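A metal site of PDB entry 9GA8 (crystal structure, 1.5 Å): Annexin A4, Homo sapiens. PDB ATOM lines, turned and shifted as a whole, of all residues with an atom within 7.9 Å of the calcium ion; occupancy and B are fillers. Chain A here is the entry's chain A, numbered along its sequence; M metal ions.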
ATOM      1  N   ARG A  96       3.064  16.993 -18.289  1.00  0.00           N
ATOM      2  CA  ARG A  96       4.218  16.619 -19.110  1.00  0.00           C
ATOM      3  C   ARG A  96       4.755  15.235 -18.717  1.00  0.00           C
ATOM      4  O   ARG A  96       5.042  14.380 -19.554  1.00  0.00           O
ATOM      5  CB  ARG A  96       5.290  17.725 -19.021  1.00  0.00           C
ATOM      6  CG  ARG A  96       6.464  17.444 -19.982  1.00  0.00           C
ATOM      7  CD  ARG A  96       6.127  17.942 -21.366  1.00  0.00           C
ATOM      8  NE  ARG A  96       6.950  17.333 -22.412  1.00  0.00           N
ATOM      9  CZ  ARG A  96       6.546  16.317 -23.209  1.00  0.00           C
ATOM     10  NH1 ARG A  96       5.259  15.979 -23.355  1.00  0.00           N
ATOM     11  NH2 ARG A  96       7.471  15.687 -23.915  1.00  0.00           N
ATOM     12  N   ARG A  97       4.969  15.011 -17.434  1.00  0.00           N
ATOM     13  CA  ARG A  97       5.499  13.760 -16.930  1.00  0.00           C
ATOM     14  C   ARG A  97       4.625  12.587 -17.342  1.00  0.00           C
ATOM     15  O   ARG A  97       5.095  11.471 -17.586  1.00  0.00           O
ATOM     16  CB  ARG A  97       5.580  13.903 -15.408  1.00  0.00           C
ATOM     17  CG  ARG A  97       6.381  12.819 -14.725  1.00  0.00           C
ATOM     18  CD  ARG A  97       6.781  13.414 -13.387  1.00  0.00           C
ATOM     19  NE  ARG A  97       7.099  12.268 -12.530  1.00  0.00           N
ATOM     20  CZ  ARG A  97       6.441  11.866 -11.463  1.00  0.00           C
ATOM     21  NH1 ARG A  97       5.319  12.460 -11.066  1.00  0.00           N
ATOM     22  NH2 ARG A  97       6.976  10.870 -10.784  1.00  0.00           N
ATOM     23  N   ALA A  98       3.323  12.830 -17.328  1.00  0.00           N
ATOM     24  CA  ALA A  98       2.348  11.808 -17.649  1.00  0.00           C
ATOM     25  C   ALA A  98       2.450  11.391 -19.117  1.00  0.00           C
ATOM     26  O   ALA A  98       2.017  10.304 -19.441  1.00  0.00           O
ATOM     27  CB  ALA A  98       0.956  12.302 -17.321  1.00  0.00           C
ATOM     28  N   MET A  99       2.984  12.239 -19.992  1.00  0.00           N
ATOM     29  CA  MET A  99       2.989  11.969 -21.422  1.00  0.00           C
ATOM     30  C   MET A  99       4.384  11.703 -21.961  1.00  0.00           C
ATOM     31  O   MET A  99       4.495  11.192 -23.077  1.00  0.00           O
ATOM     32  CB  MET A  99       2.369  13.140 -22.169  1.00  0.00           C
ATOM     33  CG  MET A  99       0.872  13.155 -21.964  1.00  0.00           C
ATOM     34  SD  MET A  99      -0.066  14.390 -22.862  1.00  0.00           S
ATOM     35  CE  MET A  99       0.322  15.899 -21.979  1.00  0.00           C
ATOM     36  N   LYS A 100       5.428  12.012 -21.186  1.00  0.00           N
ATOM     37  CA  LYS A 100       6.788  11.919 -21.690  1.00  0.00           C
ATOM     38  C   LYS A 100       7.183  10.453 -21.846  1.00  0.00           C
ATOM     39  O   LYS A 100       6.998   9.652 -20.938  1.00  0.00           O
ATOM     40  CB  LYS A 100       7.763  12.640 -20.750  1.00  0.00           C
ATOM     41  CG  LYS A 100       8.995  13.198 -21.470  1.00  0.00           C
ATOM     42  CD  LYS A 100       9.783  14.191 -20.631  1.00  0.00           C
ATOM     43  CE  LYS A 100      10.515  15.169 -21.473  1.00  0.00           C
ATOM     44  NZ  LYS A 100      11.315  14.501 -22.510  1.00  0.00           N
ATOM     45  N   GLY A 101       7.770  10.122 -23.013  1.00  0.00           N
ATOM     46  CA  GLY A 101       8.137   8.760 -23.354  1.00  0.00           C
ATOM     47  C   GLY A 101       7.032   8.037 -24.134  1.00  0.00           C
ATOM     48  O   GLY A 101       5.960   8.605 -24.387  1.00  0.00           O
ATOM     49  N   ALA A 102       7.318   6.758 -24.465  1.00  0.00           N
ATOM     50  CA  ALA A 102       6.364   5.851 -25.085  1.00  0.00           C
ATOM     51  C   ALA A 102       5.139   5.545 -24.224  1.00  0.00           C
ATOM     52  O   ALA A 102       4.085   5.268 -24.776  1.00  0.00           O
ATOM     53  CB  ALA A 102       7.072   4.557 -25.506  1.00  0.00           C
ATOM     54  N   GLY A 103       5.235   5.594 -22.891  1.00  0.00           N
ATOM     55  CA  GLY A 103       4.074   5.289 -22.048  1.00  0.00           C
ATOM     56  C   GLY A 103       3.166   6.522 -21.840  1.00  0.00           C
ATOM     57  O   GLY A 103       3.437   7.608 -22.341  1.00  0.00           O
ATOM     58  N   THR A 104       2.053   6.314 -21.118  1.00  0.00           N
ATOM     59  CA  THR A 104       1.181   7.403 -20.680  1.00  0.00           C
ATOM     60  C   THR A 104       0.635   7.099 -19.288  1.00  0.00           C
ATOM     61  O   THR A 104       0.067   6.030 -19.088  1.00  0.00           O
ATOM     62  CB  THR A 104      -0.008   7.553 -21.632  1.00  0.00           C
ATOM     63  OG1 THR A 104       0.586   7.749 -22.907  1.00  0.00           O
ATOM     64  CG2 THR A 104      -0.884   8.755 -21.308  1.00  0.00           C
ATOM     65  N   ASP A 105       0.650   8.093 -18.401  1.00  0.00           N
ATOM     66  CA  ASP A 105      -0.117   8.004 -17.159  1.00  0.00           C
ATOM     67  C   ASP A 105      -1.538   8.546 -17.359  1.00  0.00           C
ATOM     68  O   ASP A 105      -1.831   9.695 -17.041  1.00  0.00           O
ATOM     69  CB  ASP A 105       0.617   8.749 -16.053  1.00  0.00           C
ATOM     70  CG  ASP A 105       0.027   8.651 -14.664  1.00  0.00           C
ATOM     71  OD1 ASP A 105      -1.081   8.091 -14.558  1.00  0.00           O
ATOM     72  OD2 ASP A 105       0.678   9.053 -13.693  1.00  0.00           O
ATOM     73  N   ASP A 139      -0.310  17.006 -27.647  1.00  0.00           N
ATOM     74  CA  ASP A 139       0.291  15.939 -26.870  1.00  0.00           C
ATOM     75  C   ASP A 139      -0.740  14.947 -26.349  1.00  0.00           C
ATOM     76  O   ASP A 139      -0.523  13.738 -26.377  1.00  0.00           O
ATOM     77  CB  ASP A 139       1.192  16.530 -25.786  1.00  0.00           C
ATOM     78  CG  ASP A 139       2.492  17.090 -26.337  1.00  0.00           C
ATOM     79  OD1 ASP A 139       2.748  16.873 -27.549  1.00  0.00           O
ATOM     80  OD2 ASP A 139       3.154  17.785 -25.593  1.00  0.00           O
ATOM     81  N   SER A 142      -1.820  12.738 -29.076  1.00  0.00           N
ATOM     82  CA  SER A 142      -0.840  11.707 -29.407  1.00  0.00           C
ATOM     83  C   SER A 142      -0.798  10.544 -28.429  1.00  0.00           C
ATOM     84  O   SER A 142      -0.367   9.448 -28.771  1.00  0.00           O
ATOM     85  CB  SER A 142       0.559  12.275 -29.522  1.00  0.00           C
ATOM     86  OG  SER A 142       0.653  13.081 -30.681  1.00  0.00           O
ATOM     87  N   ASP A 143      -1.101  10.831 -27.162  1.00  0.00           N
ATOM     88  CA  ASP A 143      -0.877   9.901 -26.092  1.00  0.00           C
ATOM     89  C   ASP A 143      -2.105   9.072 -25.768  1.00  0.00           C
ATOM     90  O   ASP A 143      -2.020   8.233 -24.890  1.00  0.00           O
ATOM     91  CB  ASP A 143      -0.439  10.661 -24.841  1.00  0.00           C
ATOM     92  CG  ASP A 143       1.028  10.396 -24.596  1.00  0.00           C
ATOM     93  OD1 ASP A 143       1.802  10.706 -25.531  1.00  0.00           O
ATOM     94  OD2 ASP A 143       1.344   9.765 -23.551  1.00  0.00           O
ATOM     95  N   THR A 144      -3.246   9.388 -26.405  1.00  0.00           N
ATOM     96  CA  THR A 144      -4.493   8.704 -26.142  1.00  0.00           C
ATOM     97  C   THR A 144      -5.205   8.412 -27.458  1.00  0.00           C
ATOM     98  O   THR A 144      -4.857   9.004 -28.453  1.00  0.00           O
ATOM     99  CB  THR A 144      -5.349   9.570 -25.225  1.00  0.00           C
ATOM    100  OG1 THR A 144      -5.700  10.764 -25.885  1.00  0.00           O
ATOM    101  CG2 THR A 144      -4.625   9.909 -23.946  1.00  0.00           C
HETATM  102 CA    CA M   1       3.659   9.152 -24.186  1.00  0.00          CA
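The backbone carbonyl oxygen (O) of Asp 143 sits close to the side-chain hydroxyl (OG1) of Thr 104, 3.3 Å away.
Residues that only touch the calcium ion: Thr 104 and Ala 102. Within 4 Å of the calcium ion: Met 99, Gly 101, Ala 102, Gly 103, Thr 104 and Asp 143.
The calcium ion is bound by O of Gly 101 (2.4 Å), O of Gly 103 (2.4 Å), O of Met 99 (2.5 Å), OD2 of Asp 143 (2.5 Å) and OD1 of Asp 143 (2.8 Å).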
